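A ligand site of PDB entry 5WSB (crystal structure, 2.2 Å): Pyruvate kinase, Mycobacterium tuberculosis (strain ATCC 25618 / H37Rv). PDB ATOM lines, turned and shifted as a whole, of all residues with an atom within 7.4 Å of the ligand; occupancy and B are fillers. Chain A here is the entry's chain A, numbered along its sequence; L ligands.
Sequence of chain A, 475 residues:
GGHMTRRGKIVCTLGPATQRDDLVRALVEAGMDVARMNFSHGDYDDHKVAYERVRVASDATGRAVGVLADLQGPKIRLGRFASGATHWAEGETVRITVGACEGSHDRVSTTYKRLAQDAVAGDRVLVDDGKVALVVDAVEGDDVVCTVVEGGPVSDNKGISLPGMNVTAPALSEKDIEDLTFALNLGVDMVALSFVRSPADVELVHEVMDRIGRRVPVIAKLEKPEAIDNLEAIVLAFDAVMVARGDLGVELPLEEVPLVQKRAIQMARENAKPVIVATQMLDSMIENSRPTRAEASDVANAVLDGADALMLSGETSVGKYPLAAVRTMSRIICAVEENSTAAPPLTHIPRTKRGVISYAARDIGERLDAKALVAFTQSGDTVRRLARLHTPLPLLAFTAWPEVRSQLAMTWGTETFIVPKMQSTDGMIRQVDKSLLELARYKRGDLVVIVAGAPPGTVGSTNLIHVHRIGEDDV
An oxygen (O7) of the ligand is in hydrogen-bond range of the side-chain hydroxyl (OG1) of Thr 352, 3.0 Å away. The side-chain amide oxygen of Asn 271 sits close to an oxygen (O5) of the ligand (3.4 Å). A ring nitrogen (NE2) of His 348 sits at hydrogen-bond distance from an oxygen (O9) of the ligand (2.4 Å). N of Arg 351 is in hydrogen-bond range of O8 of the ligand. An oxygen (O1) of the ligand lies within hydrogen-bond range of the backbone carbonyl oxygen (O) of Asn 271 (2.7 Å). O8 of the ligand is in hydrogen-bond range of N of Thr 352, 3.5 Å away. NH1 of Arg 388 is in salt-bridge range of O9 of the ligand. NH1 of Arg 385 is in salt-bridge range of O7 of the ligand (3.1 Å).
N of Lys 273 is in hydrogen-bond range of O of Ala 268, 2.9 Å away. OE2 of Glu 270 lies within hydrogen-bond range of ND1 of His 348 (2.6 Å). OG1 of Thr 352 is in hydrogen-bond range of N of Gly 355 (3.0 Å). O of Gly 355 is in hydrogen-bond range of OG of Ser 358. O of Leu 236 lies within hydrogen-bond range of NZ of Lys 273. O of Val 235 sits at hydrogen-bond distance from NZ of Lys 273 (2.8 Å). The guanidinium group of Arg 388 is in hydrogen-bond range of the backbone carbonyl oxygen of Glu 270 (3.2 Å). NE of Arg 385 lies within salt-bridge range of OD1 of Asp 381.
Merely in contact with the ligand: Leu 236 (3.7 Å), Glu 270 (3.6 Å), Lys 273 (3.9 Å), Pro 350 (3.96 Å) and Gly 355 (3.7 Å). Of the 24 residues printed, 11 come within 4 Å of the ligand. The nearest printed residue that does not touch the ligand is Ile 349 (4.8 Å).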
ATOM      1  N   GLU A 232      -6.760  13.224 -10.142  1.00  0.00           N
ATOM      2  CA  GLU A 232      -6.637  13.588 -11.537  1.00  0.00           C
ATOM      3  C   GLU A 232      -7.855  13.105 -12.329  1.00  0.00           C
ATOM      4  O   GLU A 232      -8.376  13.840 -13.150  1.00  0.00           O
ATOM      5  CB  GLU A 232      -5.353  13.078 -12.190  1.00  0.00           C
ATOM      6  CG  GLU A 232      -5.131  13.748 -13.560  1.00  0.00           C
ATOM      7  CD  GLU A 232      -4.058  13.111 -14.433  1.00  0.00           C
ATOM      8  OE1 GLU A 232      -3.629  13.765 -15.417  1.00  0.00           O
ATOM      9  OE2 GLU A 232      -3.642  11.955 -14.173  1.00  0.00           O
ATOM     10  N   VAL A 235     -10.960  15.240 -11.436  1.00  0.00           N
ATOM     11  CA  VAL A 235     -10.828  16.567 -12.054  1.00  0.00           C
ATOM     12  C   VAL A 235     -11.131  16.539 -13.543  1.00  0.00           C
ATOM     13  O   VAL A 235     -11.654  17.514 -14.076  1.00  0.00           O
ATOM     14  CB  VAL A 235      -9.440  17.204 -11.821  1.00  0.00           C
ATOM     15  CG1 VAL A 235      -9.317  18.512 -12.598  1.00  0.00           C
ATOM     16  CG2 VAL A 235      -9.202  17.468 -10.321  1.00  0.00           C
ATOM     17  N   LEU A 236     -10.810  15.429 -14.210  1.00  0.00           N
ATOM     18  CA  LEU A 236     -10.987  15.332 -15.661  1.00  0.00           C
ATOM     19  C   LEU A 236     -12.421  14.919 -16.056  1.00  0.00           C
ATOM     20  O   LEU A 236     -12.885  15.297 -17.125  1.00  0.00           O
ATOM     21  CB  LEU A 236      -9.997  14.327 -16.268  1.00  0.00           C
ATOM     22  CG  LEU A 236      -8.545  14.810 -16.436  1.00  0.00           C
ATOM     23  CD1 LEU A 236      -7.602  13.619 -16.653  1.00  0.00           C
ATOM     24  CD2 LEU A 236      -8.426  15.778 -17.586  1.00  0.00           C
ATOM     25  N   MET A 267      -4.066  21.073  -9.593  1.00  0.00           N
ATOM     26  CA  MET A 267      -4.529  20.061 -10.533  1.00  0.00           C
ATOM     27  C   MET A 267      -5.746  20.592 -11.327  1.00  0.00           C
ATOM     28  O   MET A 267      -5.870  20.370 -12.517  1.00  0.00           O
ATOM     29  CB  MET A 267      -4.872  18.802  -9.746  1.00  0.00           C
ATOM     30  CG  MET A 267      -5.438  17.668 -10.558  1.00  0.00           C
ATOM     31  SD  MET A 267      -4.224  16.938 -11.624  1.00  0.00           S
ATOM     32  CE  MET A 267      -3.250  16.036 -10.398  1.00  0.00           C
ATOM     33  N   ALA A 268      -6.610  21.320 -10.659  1.00  0.00           N
ATOM     34  CA  ALA A 268      -7.678  22.012 -11.319  1.00  0.00           C
ATOM     35  C   ALA A 268      -7.112  22.966 -12.365  1.00  0.00           C
ATOM     36  O   ALA A 268      -7.520  22.955 -13.515  1.00  0.00           O
ATOM     37  CB  ALA A 268      -8.520  22.783 -10.303  1.00  0.00           C
ATOM     38  N   ARG A 269      -6.181  23.822 -11.981  1.00  0.00           N
ATOM     39  CA  ARG A 269      -5.664  24.800 -12.909  1.00  0.00           C
ATOM     40  C   ARG A 269      -4.892  24.154 -14.078  1.00  0.00           C
ATOM     41  O   ARG A 269      -4.922  24.683 -15.184  1.00  0.00           O
ATOM     42  CB  ARG A 269      -4.768  25.795 -12.207  1.00  0.00           C
ATOM     43  CG  ARG A 269      -5.430  26.687 -11.192  1.00  0.00           C
ATOM     44  CD  ARG A 269      -4.359  27.538 -10.498  1.00  0.00           C
ATOM     45  NE  ARG A 269      -3.538  28.212 -11.485  1.00  0.00           N
ATOM     46  CZ  ARG A 269      -2.214  28.127 -11.597  1.00  0.00           C
ATOM     47  NH1 ARG A 269      -1.492  27.418 -10.712  1.00  0.00           N
ATOM     48  NH2 ARG A 269      -1.598  28.778 -12.584  1.00  0.00           N
ATOM     49  N   GLU A 270      -4.245  23.012 -13.848  1.00  0.00           N
ATOM     50  CA  GLU A 270      -3.510  22.340 -14.927  1.00  0.00           C
ATOM     51  C   GLU A 270      -4.457  21.876 -16.015  1.00  0.00           C
ATOM     52  O   GLU A 270      -4.073  21.751 -17.172  1.00  0.00           O
ATOM     53  CB  GLU A 270      -2.732  21.108 -14.434  1.00  0.00           C
ATOM     54  CG  GLU A 270      -1.626  21.401 -13.436  1.00  0.00           C
ATOM     55  CD  GLU A 270      -0.325  21.833 -14.100  1.00  0.00           C
ATOM     56  OE1 GLU A 270       0.566  22.270 -13.365  1.00  0.00           O
ATOM     57  OE2 GLU A 270      -0.185  21.730 -15.322  1.00  0.00           O
ATOM     58  N   ASN A 271      -5.701  21.584 -15.633  1.00  0.00           N
ATOM     59  CA  ASN A 271      -6.678  21.030 -16.539  1.00  0.00           C
ATOM     60  C   ASN A 271      -7.817  22.006 -16.839  1.00  0.00           C
ATOM     61  O   ASN A 271      -8.844  21.629 -17.457  1.00  0.00           O
ATOM     62  CB  ASN A 271      -7.222  19.706 -15.992  1.00  0.00           C
ATOM     63  CG  ASN A 271      -6.171  18.614 -15.934  1.00  0.00           C
ATOM     64  OD1 ASN A 271      -5.719  18.079 -16.955  1.00  0.00           O
ATOM     65  ND2 ASN A 271      -5.789  18.265 -14.739  1.00  0.00           N
ATOM     66  N   ALA A 272      -7.605  23.269 -16.447  1.00  0.00           N
ATOM     67  CA  ALA A 272      -8.523  24.360 -16.764  1.00  0.00           C
ATOM     68  C   ALA A 272      -9.912  24.104 -16.218  1.00  0.00           C
ATOM     69  O   ALA A 272     -10.940  24.341 -16.904  1.00  0.00           O
ATOM     70  CB  ALA A 272      -8.585  24.559 -18.285  1.00  0.00           C
ATOM     71  N   LYS A 273      -9.960  23.634 -14.981  1.00  0.00           N
ATOM     72  CA  LYS A 273     -11.219  23.468 -14.290  1.00  0.00           C
ATOM     73  C   LYS A 273     -11.273  24.392 -13.117  1.00  0.00           C
ATOM     74  O   LYS A 273     -10.257  24.566 -12.420  1.00  0.00           O
ATOM     75  CB  LYS A 273     -11.423  22.023 -13.844  1.00  0.00           C
ATOM     76  CG  LYS A 273     -11.176  21.006 -14.968  1.00  0.00           C
ATOM     77  CD  LYS A 273     -12.275  21.005 -16.012  1.00  0.00           C
ATOM     78  CE  LYS A 273     -12.060  19.895 -16.998  1.00  0.00           C
ATOM     79  NZ  LYS A 273     -12.565  18.597 -16.470  1.00  0.00           N
ATOM     80  N   LEU A 346       2.250  26.621 -14.206  1.00  0.00           N
ATOM     81  CA  LEU A 346       1.840  25.307 -14.631  1.00  0.00           C
ATOM     82  C   LEU A 346       3.075  24.464 -14.864  1.00  0.00           C
ATOM     83  O   LEU A 346       4.088  24.975 -15.334  1.00  0.00           O
ATOM     84  CB  LEU A 346       1.039  25.389 -15.948  1.00  0.00           C
ATOM     85  CG  LEU A 346      -0.253  26.230 -15.864  1.00  0.00           C
ATOM     86  CD1 LEU A 346      -1.024  26.154 -17.188  1.00  0.00           C
ATOM     87  CD2 LEU A 346      -1.136  25.773 -14.725  1.00  0.00           C
ATOM     88  N   HIS A 348       3.330  22.136 -17.104  1.00  0.00           N
ATOM     89  CA  HIS A 348       3.413  21.706 -18.490  1.00  0.00           C
ATOM     90  C   HIS A 348       3.238  22.877 -19.444  1.00  0.00           C
ATOM     91  O   HIS A 348       2.629  23.897 -19.098  1.00  0.00           O
ATOM     92  CB  HIS A 348       2.386  20.613 -18.803  1.00  0.00           C
ATOM     93  CG  HIS A 348       0.990  21.121 -18.926  1.00  0.00           C
ATOM     94  ND1 HIS A 348       0.193  21.404 -17.847  1.00  0.00           N
ATOM     95  CD2 HIS A 348       0.257  21.448 -20.011  1.00  0.00           C
ATOM     96  CE1 HIS A 348      -0.954  21.914 -18.259  1.00  0.00           C
ATOM     97  NE2 HIS A 348      -0.942  21.959 -19.566  1.00  0.00           N
ATOM     98  N   ILE A 349       3.826  22.738 -20.628  1.00  0.00           N
ATOM     99  CA  ILE A 349       3.580  23.624 -21.733  1.00  0.00           C
ATOM    100  C   ILE A 349       2.215  23.244 -22.324  1.00  0.00           C
ATOM    101  O   ILE A 349       1.947  22.069 -22.526  1.00  0.00           O
ATOM    102  CB  ILE A 349       4.589  23.385 -22.902  1.00  0.00           C
ATOM    103  CG1 ILE A 349       6.045  23.372 -22.415  1.00  0.00           C
ATOM    104  CG2 ILE A 349       4.376  24.443 -23.957  1.00  0.00           C
ATOM    105  CD1 ILE A 349       6.496  24.679 -21.828  1.00  0.00           C
ATOM    106  N   PRO A 350       1.381  24.238 -22.642  1.00  0.00           N
ATOM    107  CA  PRO A 350       0.057  23.923 -23.239  1.00  0.00           C
ATOM    108  C   PRO A 350       0.163  23.218 -24.590  1.00  0.00           C
ATOM    109  O   PRO A 350       1.055  23.530 -25.413  1.00  0.00           O
ATOM    110  CB  PRO A 350      -0.625  25.280 -23.332  1.00  0.00           C
ATOM    111  CG  PRO A 350       0.007  26.076 -22.224  1.00  0.00           C
ATOM    112  CD  PRO A 350       1.432  25.614 -22.103  1.00  0.00           C
ATOM    113  N   ARG A 351      -0.705  22.224 -24.786  1.00  0.00           N
ATOM    114  CA  ARG A 351      -0.788  21.483 -26.067  1.00  0.00           C
ATOM    115  C   ARG A 351      -2.104  21.704 -26.858  1.00  0.00           C
ATOM    116  O   ARG A 351      -2.099  21.607 -28.083  1.00  0.00           O
ATOM    117  CB  ARG A 351      -0.582  19.970 -25.837  1.00  0.00           C
ATOM    118  CG  ARG A 351      -0.436  19.146 -27.119  1.00  0.00           C
ATOM    119  CD  ARG A 351       0.332  17.840 -26.906  1.00  0.00           C
ATOM    120  NE  ARG A 351       1.499  18.014 -26.025  1.00  0.00           N
ATOM    121  CZ  ARG A 351       2.779  17.899 -26.398  1.00  0.00           C
ATOM    122  NH1 ARG A 351       3.115  17.569 -27.646  1.00  0.00           N
ATOM    123  NH2 ARG A 351       3.723  18.112 -25.508  1.00  0.00           N
ATOM    124  N   THR A 352      -3.232  21.914 -26.168  1.00  0.00           N
ATOM    125  CA  THR A 352      -4.501  22.056 -26.884  1.00  0.00           C
ATOM    126  C   THR A 352      -4.529  23.416 -27.530  1.00  0.00           C
ATOM    127  O   THR A 352      -3.989  24.383 -26.983  1.00  0.00           O
ATOM    128  CB  THR A 352      -5.740  21.991 -25.973  1.00  0.00           C
ATOM    129  OG1 THR A 352      -5.832  23.184 -25.163  1.00  0.00           O
ATOM    130  CG2 THR A 352      -5.683  20.739 -25.099  1.00  0.00           C
ATOM    131  N   LYS A 353      -5.187  23.490 -28.672  1.00  0.00           N
ATOM    132  CA  LYS A 353      -5.267  24.712 -29.443  1.00  0.00           C
ATOM    133  C   LYS A 353      -5.719  25.852 -28.585  1.00  0.00           C
ATOM    134  O   LYS A 353      -5.167  26.950 -28.662  1.00  0.00           O
ATOM    135  CB  LYS A 353      -6.249  24.512 -30.616  1.00  0.00           C
ATOM    136  CG  LYS A 353      -6.317  25.712 -31.554  1.00  0.00           C
ATOM    137  CD  LYS A 353      -7.110  25.427 -32.820  1.00  0.00           C
ATOM    138  CE  LYS A 353      -8.519  24.987 -32.490  1.00  0.00           C
ATOM    139  NZ  LYS A 353      -9.464  25.143 -33.616  1.00  0.00           N
ATOM    140  N   ARG A 354      -6.757  25.612 -27.793  1.00  0.00           N
ATOM    141  CA  ARG A 354      -7.356  26.661 -26.972  1.00  0.00           C
ATOM    142  C   ARG A 354      -6.427  27.102 -25.845  1.00  0.00           C
ATOM    143  O   ARG A 354      -6.406  28.299 -25.465  1.00  0.00           O
ATOM    144  CB  ARG A 354      -8.683  26.181 -26.372  1.00  0.00           C
ATOM    145  CG  ARG A 354      -9.879  26.420 -27.311  1.00  0.00           C
ATOM    146  CD  ARG A 354     -11.151  25.776 -26.790  1.00  0.00           C
ATOM    147  NE  ARG A 354     -10.989  24.332 -26.714  1.00  0.00           N
ATOM    148  CZ  ARG A 354     -11.953  23.481 -26.376  1.00  0.00           C
ATOM    149  NH1 ARG A 354     -13.150  23.920 -26.090  1.00  0.00           N
ATOM    150  NH2 ARG A 354     -11.686  22.184 -26.317  1.00  0.00           N
ATOM    151  N   GLY A 355      -5.656  26.145 -25.329  1.00  0.00           N
ATOM    152  CA  GLY A 355      -4.699  26.438 -24.279  1.00  0.00           C
ATOM    153  C   GLY A 355      -3.544  27.268 -24.809  1.00  0.00           C
ATOM    154  O   GLY A 355      -3.160  28.279 -24.217  1.00  0.00           O
ATOM    155  N   VAL A 356      -2.990  26.841 -25.931  1.00  0.00           N
ATOM    156  CA  VAL A 356      -1.860  27.511 -26.532  1.00  0.00           C
ATOM    157  C   VAL A 356      -2.224  28.915 -26.960  1.00  0.00           C
ATOM    158  O   VAL A 356      -1.431  29.852 -26.777  1.00  0.00           O
ATOM    159  CB  VAL A 356      -1.387  26.731 -27.742  1.00  0.00           C
ATOM    160  CG1 VAL A 356      -0.560  27.594 -28.690  1.00  0.00           C
ATOM    161  CG2 VAL A 356      -0.668  25.465 -27.302  1.00  0.00           C
ATOM    162  N   SER A 358      -4.895  30.827 -25.911  1.00  0.00           N
ATOM    163  CA  SER A 358      -5.156  31.676 -24.738  1.00  0.00           C
ATOM    164  C   SER A 358      -3.848  32.067 -23.995  1.00  0.00           C
ATOM    165  O   SER A 358      -3.721  33.181 -23.442  1.00  0.00           O
ATOM    166  CB  SER A 358      -6.122  30.961 -23.789  1.00  0.00           C
ATOM    167  OG  SER A 358      -5.572  29.743 -23.318  1.00  0.00           O
ATOM    168  N   ASP A 381     -14.614  27.259 -22.104  1.00  0.00           N
ATOM    169  CA  ASP A 381     -13.336  26.580 -22.002  1.00  0.00           C
ATOM    170  C   ASP A 381     -12.194  27.503 -22.355  1.00  0.00           C
ATOM    171  O   ASP A 381     -11.186  27.555 -21.659  1.00  0.00           O
ATOM    172  CB  ASP A 381     -13.352  25.371 -22.926  1.00  0.00           C
ATOM    173  CG  ASP A 381     -12.096  24.577 -22.853  1.00  0.00           C
ATOM    174  OD1 ASP A 381     -11.109  24.985 -23.522  1.00  0.00           O
ATOM    175  OD2 ASP A 381     -12.103  23.493 -22.155  1.00  0.00           O
ATOM    176  N   ARG A 385      -9.036  28.514 -19.849  1.00  0.00           N
ATOM    177  CA  ARG A 385      -7.629  28.280 -20.111  1.00  0.00           C
ATOM    178  C   ARG A 385      -6.777  29.519 -19.967  1.00  0.00           C
ATOM    179  O   ARG A 385      -5.546  29.397 -19.740  1.00  0.00           O
ATOM    180  CB  ARG A 385      -7.432  27.642 -21.476  1.00  0.00           C
ATOM    181  CG  ARG A 385      -8.030  26.266 -21.484  1.00  0.00           C
ATOM    182  CD  ARG A 385      -7.714  25.456 -22.718  1.00  0.00           C
ATOM    183  NE  ARG A 385      -8.619  24.328 -22.695  1.00  0.00           N
ATOM    184  CZ  ARG A 385      -8.405  23.199 -22.036  1.00  0.00           C
ATOM    185  NH1 ARG A 385      -7.244  23.035 -21.392  1.00  0.00           N
ATOM    186  NH2 ARG A 385      -9.339  22.231 -22.020  1.00  0.00           N
ATOM    187  N   ARG A 388      -6.911  30.579 -15.708  1.00  0.00           N
ATOM    188  CA  ARG A 388      -6.090  29.743 -14.848  1.00  0.00           C
ATOM    189  C   ARG A 388      -4.692  30.344 -14.742  1.00  0.00           C
ATOM    190  O   ARG A 388      -4.022  30.162 -13.736  1.00  0.00           O
ATOM    191  CB  ARG A 388      -6.022  28.317 -15.410  1.00  0.00           C
ATOM    192  CG  ARG A 388      -5.246  28.208 -16.693  1.00  0.00           C
ATOM    193  CD  ARG A 388      -5.246  26.804 -17.251  1.00  0.00           C
ATOM    194  NE  ARG A 388      -4.726  26.763 -18.614  1.00  0.00           N
ATOM    195  CZ  ARG A 388      -4.398  25.653 -19.288  1.00  0.00           C
ATOM    196  NH1 ARG A 388      -4.484  24.477 -18.715  1.00  0.00           N
ATOM    197  NH2 ARG A 388      -3.962  25.725 -20.541  1.00  0.00           N
HETATM  198  C1  LIG L   1      -8.013  19.580 -20.376  1.00  0.00           C
HETATM  199  C2  LIG L   1      -8.215  18.308 -21.184  1.00  0.00           C
HETATM  200  C3  LIG L   1      -7.020  17.394 -21.205  1.00  0.00           C
HETATM  201  C4  LIG L   1      -5.758  18.219 -21.373  1.00  0.00           C
HETATM  202  C5  LIG L   1      -5.578  19.074 -20.157  1.00  0.00           C
HETATM  203  C6  LIG L   1      -4.494  20.119 -20.350  1.00  0.00           C
HETATM  204  O1  LIG L   1      -9.027  19.666 -19.370  1.00  0.00           O
HETATM  205  O2  LIG L   1      -9.354  17.608 -20.659  1.00  0.00           O
HETATM  206  O3  LIG L   1      -7.151  16.462 -22.289  1.00  0.00           O
HETATM  207  O4  LIG L   1      -4.627  17.366 -21.456  1.00  0.00           O
HETATM  208  O5  LIG L   1      -6.756  19.745 -19.712  1.00  0.00           O
HETATM  209  O6  LIG L   1      -4.879  21.047 -21.340  1.00  0.00           O
HETATM  210  P1  LIG L   1      -3.745  22.047 -21.883  1.00  0.00           P
HETATM  211  O7  LIG L   1      -4.368  23.224 -22.572  1.00  0.00           O
HETATM  212  O8  LIG L   1      -2.825  21.246 -22.783  1.00  0.00           O
HETATM  213  O9  LIG L   1      -3.026  22.579 -20.683  1.00  0.00           O
